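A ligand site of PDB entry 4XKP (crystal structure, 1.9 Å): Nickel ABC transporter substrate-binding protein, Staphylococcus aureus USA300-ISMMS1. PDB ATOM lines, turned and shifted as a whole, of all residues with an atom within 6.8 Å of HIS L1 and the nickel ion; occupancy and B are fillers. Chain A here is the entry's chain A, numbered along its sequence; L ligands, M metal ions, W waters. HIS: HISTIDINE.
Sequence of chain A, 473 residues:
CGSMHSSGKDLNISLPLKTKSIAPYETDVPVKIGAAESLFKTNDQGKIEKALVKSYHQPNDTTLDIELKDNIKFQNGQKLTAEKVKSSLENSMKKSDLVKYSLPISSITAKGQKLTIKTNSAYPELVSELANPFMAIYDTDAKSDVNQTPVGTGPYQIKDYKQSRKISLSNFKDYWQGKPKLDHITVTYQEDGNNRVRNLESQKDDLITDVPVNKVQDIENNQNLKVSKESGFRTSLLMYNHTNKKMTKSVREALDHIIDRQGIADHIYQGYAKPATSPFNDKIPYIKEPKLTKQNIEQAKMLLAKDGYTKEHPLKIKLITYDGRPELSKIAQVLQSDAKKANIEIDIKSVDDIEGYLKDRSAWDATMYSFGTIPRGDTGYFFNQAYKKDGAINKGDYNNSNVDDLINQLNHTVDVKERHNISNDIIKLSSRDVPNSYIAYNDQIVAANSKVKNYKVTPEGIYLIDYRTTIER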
ATOM      1  N   PRO A  16     -19.699 -25.290  -7.264  1.00  0.00           N
ATOM      2  CA  PRO A  16     -20.169 -24.966  -5.923  1.00  0.00           C
ATOM      3  C   PRO A  16     -20.852 -23.595  -5.899  1.00  0.00           C
ATOM      4  O   PRO A  16     -20.913 -22.901  -6.913  1.00  0.00           O
ATOM      5  CB  PRO A  16     -18.889 -24.949  -5.087  1.00  0.00           C
ATOM      6  CG  PRO A  16     -17.865 -24.440  -6.054  1.00  0.00           C
ATOM      7  CD  PRO A  16     -18.259 -25.000  -7.416  1.00  0.00           C
ATOM      8  N   LEU A  17     -21.345 -23.232  -4.723  1.00  0.00           N
ATOM      9  CA  LEU A  17     -21.856 -21.901  -4.407  1.00  0.00           C
ATOM     10  C   LEU A  17     -23.127 -21.593  -5.179  1.00  0.00           C
ATOM     11  O   LEU A  17     -23.167 -20.681  -6.008  1.00  0.00           O
ATOM     12  CB  LEU A  17     -20.778 -20.830  -4.680  1.00  0.00           C
ATOM     13  CG  LEU A  17     -19.484 -21.069  -3.899  1.00  0.00           C
ATOM     14  CD1 LEU A  17     -18.522 -19.909  -4.076  1.00  0.00           C
ATOM     15  CD2 LEU A  17     -19.743 -21.331  -2.410  1.00  0.00           C
ATOM     16  N   LYS A  18     -24.169 -22.375  -4.872  1.00  0.00           N
ATOM     17  CA  LYS A  18     -25.478 -22.220  -5.495  1.00  0.00           C
ATOM     18  C   LYS A  18     -25.950 -20.778  -5.401  1.00  0.00           C
ATOM     19  O   LYS A  18     -25.700 -20.085  -4.419  1.00  0.00           O
ATOM     20  CB  LYS A  18     -26.510 -23.146  -4.840  1.00  0.00           C
ATOM     21  CG  LYS A  18     -26.748 -22.874  -3.352  1.00  0.00           C
ATOM     22  CD  LYS A  18     -27.909 -23.696  -2.789  1.00  0.00           C
ATOM     23  CE  LYS A  18     -27.561 -25.165  -2.714  1.00  0.00           C
ATOM     24  NZ  LYS A  18     -28.739 -26.000  -2.330  1.00  0.00           N
ATOM     25  N   THR A  19     -26.639 -20.340  -6.451  1.00  0.00           N
ATOM     26  CA  THR A  19     -27.165 -18.991  -6.555  1.00  0.00           C
ATOM     27  C   THR A  19     -28.645 -18.979  -6.228  1.00  0.00           C
ATOM     28  O   THR A  19     -29.300 -20.014  -6.268  1.00  0.00           O
ATOM     29  CB  THR A  19     -26.982 -18.448  -7.974  1.00  0.00           C
ATOM     30  OG1 THR A  19     -27.456 -19.442  -8.893  1.00  0.00           O
ATOM     31  CG2 THR A  19     -25.509 -18.169  -8.254  1.00  0.00           C
ATOM     32  N   THR A  27     -24.416 -12.258  -9.452  1.00  0.00           N
ATOM     33  CA  THR A  27     -23.468 -13.371  -9.445  1.00  0.00           C
ATOM     34  C   THR A  27     -22.599 -13.355 -10.710  1.00  0.00           C
ATOM     35  O   THR A  27     -23.042 -12.899 -11.765  1.00  0.00           O
ATOM     36  CB  THR A  27     -24.198 -14.736  -9.328  1.00  0.00           C
ATOM     37  OG1 THR A  27     -23.288 -15.812  -9.576  1.00  0.00           O
ATOM     38  CG2 THR A  27     -25.346 -14.811 -10.318  1.00  0.00           C
ATOM     39  N   ASP A  28     -21.372 -13.853 -10.603  1.00  0.00           N
ATOM     40  CA  ASP A  28     -20.498 -13.883 -11.766  1.00  0.00           C
ATOM     41  C   ASP A  28     -20.714 -15.155 -12.591  1.00  0.00           C
ATOM     42  O   ASP A  28     -20.062 -15.356 -13.625  1.00  0.00           O
ATOM     43  CB  ASP A  28     -19.023 -13.731 -11.346  1.00  0.00           C
ATOM     44  CG  ASP A  28     -18.461 -14.984 -10.666  1.00  0.00           C
ATOM     45  OD1 ASP A  28     -19.202 -15.957 -10.412  1.00  0.00           O
ATOM     46  OD2 ASP A  28     -17.247 -14.980 -10.368  1.00  0.00           O
ATOM     47  N   PHE A 134     -19.837  -8.670 -12.624  1.00  0.00           N
ATOM     48  CA  PHE A 134     -21.108  -8.185 -12.101  1.00  0.00           C
ATOM     49  C   PHE A 134     -21.632  -7.042 -12.967  1.00  0.00           C
ATOM     50  O   PHE A 134     -22.806  -6.686 -12.878  1.00  0.00           O
ATOM     51  CB  PHE A 134     -20.959  -7.746 -10.641  1.00  0.00           C
ATOM     52  CG  PHE A 134     -20.903  -8.897  -9.675  1.00  0.00           C
ATOM     53  CD1 PHE A 134     -19.734  -9.620  -9.514  1.00  0.00           C
ATOM     54  CD2 PHE A 134     -22.012  -9.247  -8.930  1.00  0.00           C
ATOM     55  CE1 PHE A 134     -19.681 -10.695  -8.630  1.00  0.00           C
ATOM     56  CE2 PHE A 134     -21.961 -10.311  -8.037  1.00  0.00           C
ATOM     57  CZ  PHE A 134     -20.801 -11.037  -7.885  1.00  0.00           C
ATOM     58  N   ARG A 234      -7.099 -15.813  -5.271  1.00  0.00           N
ATOM     59  CA  ARG A 234      -8.132 -16.085  -4.281  1.00  0.00           C
ATOM     60  C   ARG A 234      -7.494 -16.338  -2.926  1.00  0.00           C
ATOM     61  O   ARG A 234      -6.486 -17.037  -2.810  1.00  0.00           O
ATOM     62  CB  ARG A 234      -8.990 -17.280  -4.711  1.00  0.00           C
ATOM     63  CG  ARG A 234     -10.053 -17.667  -3.687  1.00  0.00           C
ATOM     64  CD  ARG A 234     -11.191 -18.429  -4.347  1.00  0.00           C
ATOM     65  NE  ARG A 234     -11.967 -17.559  -5.222  1.00  0.00           N
ATOM     66  CZ  ARG A 234     -12.966 -16.793  -4.809  1.00  0.00           C
ATOM     67  NH1 ARG A 234     -13.333 -16.809  -3.529  1.00  0.00           N
ATOM     68  NH2 ARG A 234     -13.611 -16.031  -5.666  1.00  0.00           N
ATOM     69  N   TYR A 322     -18.758 -23.287   5.274  1.00  0.00           N
ATOM     70  CA  TYR A 322     -19.546 -23.797   4.157  1.00  0.00           C
ATOM     71  C   TYR A 322     -18.668 -24.719   3.318  1.00  0.00           C
ATOM     72  O   TYR A 322     -17.436 -24.656   3.411  1.00  0.00           O
ATOM     73  CB  TYR A 322     -20.145 -22.647   3.315  1.00  0.00           C
ATOM     74  CG  TYR A 322     -19.139 -21.638   2.779  1.00  0.00           C
ATOM     75  CD1 TYR A 322     -18.524 -20.719   3.622  1.00  0.00           C
ATOM     76  CD2 TYR A 322     -18.823 -21.602   1.421  1.00  0.00           C
ATOM     77  CE1 TYR A 322     -17.602 -19.801   3.128  1.00  0.00           C
ATOM     78  CE2 TYR A 322     -17.913 -20.677   0.927  1.00  0.00           C
ATOM     79  CZ  TYR A 322     -17.306 -19.782   1.786  1.00  0.00           C
ATOM     80  OH  TYR A 322     -16.387 -18.867   1.306  1.00  0.00           O
ATOM     81  N   GLY A 324     -18.465 -25.133  -0.113  1.00  0.00           N
ATOM     82  CA  GLY A 324     -18.128 -24.748  -1.481  1.00  0.00           C
ATOM     83  C   GLY A 324     -16.641 -24.674  -1.778  1.00  0.00           C
ATOM     84  O   GLY A 324     -16.176 -25.201  -2.790  1.00  0.00           O
ATOM     85  N   ARG A 325     -15.887 -24.023  -0.898  1.00  0.00           N
ATOM     86  CA  ARG A 325     -14.436 -24.067  -0.952  1.00  0.00           C
ATOM     87  C   ARG A 325     -14.015 -25.178   0.003  1.00  0.00           C
ATOM     88  O   ARG A 325     -14.118 -25.018   1.213  1.00  0.00           O
ATOM     89  CB  ARG A 325     -13.806 -22.718  -0.559  1.00  0.00           C
ATOM     90  CG  ARG A 325     -14.492 -21.503  -1.201  1.00  0.00           C
ATOM     91  CD  ARG A 325     -14.125 -21.319  -2.678  1.00  0.00           C
ATOM     92  NE  ARG A 325     -14.793 -20.148  -3.252  1.00  0.00           N
ATOM     93  CZ  ARG A 325     -14.866 -19.875  -4.550  1.00  0.00           C
ATOM     94  NH1 ARG A 325     -14.309 -20.691  -5.427  1.00  0.00           N
ATOM     95  NH2 ARG A 325     -15.490 -18.789  -4.978  1.00  0.00           N
ATOM     96  N   LEU A 328     -12.036 -24.957   3.584  1.00  0.00           N
ATOM     97  CA  LEU A 328     -12.439 -24.042   4.657  1.00  0.00           C
ATOM     98  C   LEU A 328     -12.900 -24.784   5.915  1.00  0.00           C
ATOM     99  O   LEU A 328     -12.521 -24.415   7.024  1.00  0.00           O
ATOM    100  CB  LEU A 328     -13.554 -23.105   4.185  1.00  0.00           C
ATOM    101  CG  LEU A 328     -13.185 -22.046   3.131  1.00  0.00           C
ATOM    102  CD1 LEU A 328     -14.393 -21.179   2.820  1.00  0.00           C
ATOM    103  CD2 LEU A 328     -12.022 -21.191   3.578  1.00  0.00           C
ATOM    104  N   ASP A 353     -26.151 -21.827   2.390  1.00  0.00           N
ATOM    105  CA  ASP A 353     -26.186 -20.553   1.681  1.00  0.00           C
ATOM    106  C   ASP A 353     -25.428 -19.508   2.482  1.00  0.00           C
ATOM    107  O   ASP A 353     -26.011 -18.795   3.301  1.00  0.00           O
ATOM    108  CB  ASP A 353     -27.647 -20.128   1.434  1.00  0.00           C
ATOM    109  CG  ASP A 353     -27.776 -18.715   0.899  1.00  0.00           C
ATOM    110  OD1 ASP A 353     -26.794 -18.185   0.351  1.00  0.00           O
ATOM    111  OD2 ASP A 353     -28.879 -18.145   1.029  1.00  0.00           O
ATOM    112  N   ILE A 354     -24.118 -19.408   2.261  1.00  0.00           N
ATOM    113  CA  ILE A 354     -23.290 -18.579   3.125  1.00  0.00           C
ATOM    114  C   ILE A 354     -23.615 -17.079   3.015  1.00  0.00           C
ATOM    115  O   ILE A 354     -23.704 -16.374   4.027  1.00  0.00           O
ATOM    116  CB  ILE A 354     -21.781 -18.831   2.828  1.00  0.00           C
ATOM    117  CG1 ILE A 354     -20.885 -18.056   3.804  1.00  0.00           C
ATOM    118  CG2 ILE A 354     -21.421 -18.545   1.360  1.00  0.00           C
ATOM    119  CD1 ILE A 354     -21.041 -18.469   5.272  1.00  0.00           C
ATOM    120  N   GLU A 355     -23.848 -16.583   1.799  1.00  0.00           N
ATOM    121  CA  GLU A 355     -24.102 -15.160   1.616  1.00  0.00           C
ATOM    122  C   GLU A 355     -25.376 -14.751   2.322  1.00  0.00           C
ATOM    123  O   GLU A 355     -25.440 -13.707   2.966  1.00  0.00           O
ATOM    124  CB  GLU A 355     -24.189 -14.798   0.127  1.00  0.00           C
ATOM    125  CG  GLU A 355     -22.879 -14.977  -0.644  1.00  0.00           C
ATOM    126  CD  GLU A 355     -21.784 -14.032  -0.172  1.00  0.00           C
ATOM    127  OE1 GLU A 355     -21.689 -12.905  -0.722  1.00  0.00           O
ATOM    128  OE2 GLU A 355     -21.017 -14.407   0.735  1.00  0.00           O
ATOM    129  N   TYR A 369     -14.173 -17.783   5.181  1.00  0.00           N
ATOM    130  CA  TYR A 369     -14.544 -17.077   3.955  1.00  0.00           C
ATOM    131  C   TYR A 369     -13.446 -17.173   2.922  1.00  0.00           C
ATOM    132  O   TYR A 369     -12.313 -17.569   3.204  1.00  0.00           O
ATOM    133  CB  TYR A 369     -14.856 -15.602   4.250  1.00  0.00           C
ATOM    134  CG  TYR A 369     -15.899 -14.993   3.313  1.00  0.00           C
ATOM    135  CD1 TYR A 369     -17.236 -15.390   3.379  1.00  0.00           C
ATOM    136  CD2 TYR A 369     -15.552 -14.030   2.386  1.00  0.00           C
ATOM    137  CE1 TYR A 369     -18.207 -14.819   2.535  1.00  0.00           C
ATOM    138  CE2 TYR A 369     -16.511 -13.467   1.543  1.00  0.00           C
ATOM    139  CZ  TYR A 369     -17.833 -13.854   1.620  1.00  0.00           C
ATOM    140  OH  TYR A 369     -18.755 -13.289   0.769  1.00  0.00           O
ATOM    141  N   SER A 370     -13.783 -16.788   1.691  1.00  0.00           N
ATOM    142  CA  SER A 370     -12.849 -16.852   0.592  1.00  0.00           C
ATOM    143  C   SER A 370     -13.192 -15.728  -0.378  1.00  0.00           C
ATOM    144  O   SER A 370     -14.370 -15.536  -0.710  1.00  0.00           O
ATOM    145  CB  SER A 370     -12.911 -18.203  -0.111  1.00  0.00           C
ATOM    146  OG  SER A 370     -12.127 -18.202  -1.292  1.00  0.00           O
ATOM    147  N   PHE A 371     -12.212 -14.985  -0.840  1.00  0.00           N
ATOM    148  CA  PHE A 371     -12.537 -13.960  -1.808  1.00  0.00           C
ATOM    149  C   PHE A 371     -11.441 -13.748  -2.826  1.00  0.00           C
ATOM    150  O   PHE A 371     -10.257 -13.974  -2.564  1.00  0.00           O
ATOM    151  CB  PHE A 371     -12.855 -12.633  -1.117  1.00  0.00           C
ATOM    152  CG  PHE A 371     -13.392 -11.587  -2.045  1.00  0.00           C
ATOM    153  CD1 PHE A 371     -14.641 -11.736  -2.621  1.00  0.00           C
ATOM    154  CD2 PHE A 371     -12.647 -10.463  -2.360  1.00  0.00           C
ATOM    155  CE1 PHE A 371     -15.143 -10.783  -3.487  1.00  0.00           C
ATOM    156  CE2 PHE A 371     -13.136  -9.504  -3.230  1.00  0.00           C
ATOM    157  CZ  PHE A 371     -14.383  -9.661  -3.785  1.00  0.00           C
ATOM    158  N   GLY A 372     -11.873 -13.324  -4.008  1.00  0.00           N
ATOM    159  CA  GLY A 372     -10.983 -13.055  -5.118  1.00  0.00           C
ATOM    160  C   GLY A 372     -10.529 -11.613  -4.892  1.00  0.00           C
ATOM    161  O   GLY A 372     -11.241 -10.685  -5.253  1.00  0.00           O
ATOM    162  N   ILE A 393     -18.759  -7.099   0.265  1.00  0.00           N
ATOM    163  CA  ILE A 393     -18.214  -8.277   0.940  1.00  0.00           C
ATOM    164  C   ILE A 393     -17.779  -7.975   2.368  1.00  0.00           C
ATOM    165  O   ILE A 393     -17.139  -8.799   3.017  1.00  0.00           O
ATOM    166  CB  ILE A 393     -17.042  -8.860   0.173  1.00  0.00           C
ATOM    167  CG1 ILE A 393     -16.219  -7.723  -0.418  1.00  0.00           C
ATOM    168  CG2 ILE A 393     -17.536  -9.800  -0.929  1.00  0.00           C
ATOM    169  CD1 ILE A 393     -14.831  -8.080  -0.797  1.00  0.00           C
ATOM    170  N   LYS A 395     -18.942  -8.309   5.231  1.00  0.00           N
ATOM    171  CA  LYS A 395     -19.997  -8.975   5.991  1.00  0.00           C
ATOM    172  C   LYS A 395     -19.948  -8.639   7.482  1.00  0.00           C
ATOM    173  O   LYS A 395     -20.992  -8.559   8.136  1.00  0.00           O
ATOM    174  CB  LYS A 395     -19.915 -10.509   5.843  1.00  0.00           C
ATOM    175  CG  LYS A 395     -19.737 -11.009   4.422  1.00  0.00           C
ATOM    176  CD  LYS A 395     -20.820 -10.495   3.484  1.00  0.00           C
ATOM    177  CE  LYS A 395     -20.727 -11.196   2.139  1.00  0.00           C
ATOM    178  NZ  LYS A 395     -21.738 -10.719   1.156  1.00  0.00           N
HETATM  179  N   HIS L   1     -17.363 -15.076  -1.413  1.00  0.00           N
HETATM  180  CA  HIS L   1     -17.411 -16.447  -0.902  1.00  0.00           C
HETATM  181  C   HIS L   1     -16.688 -17.413  -1.827  1.00  0.00           C
HETATM  182  O   HIS L   1     -16.507 -17.113  -3.003  1.00  0.00           O
HETATM  183  CB  HIS L   1     -18.871 -16.886  -0.705  1.00  0.00           C
HETATM  184  CG  HIS L   1     -19.687 -16.890  -1.953  1.00  0.00           C
HETATM  185  ND1 HIS L   1     -19.327 -16.222  -3.103  1.00  0.00           N
HETATM  186  CD2 HIS L   1     -20.877 -17.488  -2.238  1.00  0.00           C
HETATM  187  CE1 HIS L   1     -20.246 -16.397  -4.033  1.00  0.00           C
HETATM  188  NE2 HIS L   1     -21.203 -17.167  -3.535  1.00  0.00           N
HETATM  189  OXT HIS L   1     -16.259 -18.495  -1.425  1.00  0.00           O
HETATM  190  N   HIS L   2     -17.538 -15.544  -5.574  1.00  0.00           N
HETATM  191  CA  HIS L   2     -16.693 -14.407  -5.957  1.00  0.00           C
HETATM  192  C   HIS L   2     -15.643 -14.097  -4.901  1.00  0.00           C
HETATM  193  O   HIS L   2     -14.646 -13.399  -5.156  1.00  0.00           O
HETATM  194  CB  HIS L   2     -17.533 -13.160  -6.213  1.00  0.00           C
HETATM  195  CG  HIS L   2     -18.261 -12.660  -4.997  1.00  0.00           C
HETATM  196  ND1 HIS L   2     -18.409 -13.421  -3.856  1.00  0.00           N
HETATM  197  CD2 HIS L   2     -18.894 -11.485  -4.757  1.00  0.00           C
HETATM  198  CE1 HIS L   2     -19.104 -12.726  -2.965  1.00  0.00           C
HETATM  199  NE2 HIS L   2     -19.412 -11.555  -3.491  1.00  0.00           N
HETATM  200  OXT HIS L   2     -15.760 -14.543  -3.759  1.00  0.00           O
HETATM  201 NI    NI M   1     -17.522 -15.314  -3.416  1.00  0.00          NI
HETATM  202  O   HOH W   1     -23.221 -17.978  -5.309  1.00  0.00           O
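The side-chain hydroxyl of Tyr 322 lies within hydrogen-bond range of an oxygen (OXT) of HIS L1 (2.8 Å).
An oxygen (OXT) of HIS L1 is in salt-bridge range of the guanidinium group (NE) of Arg 325 (2.9 Å).
O of Ser 370 sits close to N of HIS L1 (3.1 Å).
The side-chain hydroxyl (OH) of Tyr 369 lies close to a nitrogen (N) of HIS L1, at 3.1 Å.
The guanidinium group (NH1) of Arg 234 lies within salt-bridge range of an oxygen (OXT) of HIS L1 (3.98 Å).
O of HIS L2 is in salt-bridge range of NH2 of Arg 234.
N of Gly 372 is in hydrogen-bond range of O of HIS L2 (3.0 Å).
N of Ser 370 sits at hydrogen-bond distance from OH of Tyr 322, 3.4 Å away.
OG of Ser 370 lies within hydrogen-bond range of NH1 of Arg 234, at 2.9 Å.
OE2 of Glu 355 lies within hydrogen-bond range of OH of Tyr 369, 2.5 Å away.
OE1 of Glu 355 is in salt-bridge range of NZ of Lys 395 (2.9 Å).
Leu 17 touches HIS L1.
Ile 354 touches HIS L1.
Glu 355 touches HIS L1.
Hydrophobic or aromatic side chains within 4 Å of HIS L1: Leu 17, Tyr 322, Ile 354 and Tyr 369.
Eight residues have an atom within 4 Å of HIS L1: Leu 17, Arg 234, Tyr 322, Arg 325, Ile 354, Glu 355, Tyr 369 and Ser 370.
The nearest printed residue that does not touch HIS L1 is Phe 371 (4.5 Å).
No residue comes within 4 Å of the nickel ion.
The nearest printed residue that does not touch the nickel ion is Ser 370 (4.2 Å).
The nickel ion is bound by OXT of HIS L2 (2.0 Å), N of HIS L1 (2.0 Å), ND1 of HIS L1 (2.0 Å), O of HIS L1 (2.1 Å), ND1 of HIS L2 (2.1 Å) and N of HIS L2 (2.2 Å).
Water W1 lies within hydrogen-bond range of the backbone carbonyl oxygen (O) of Leu 17 (2.8 Å), a nitrogen (NE2) of HIS L1 (2.8 Å) and the backbone carbonyl oxygen (O) of Lys 18 (3.4 Å).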
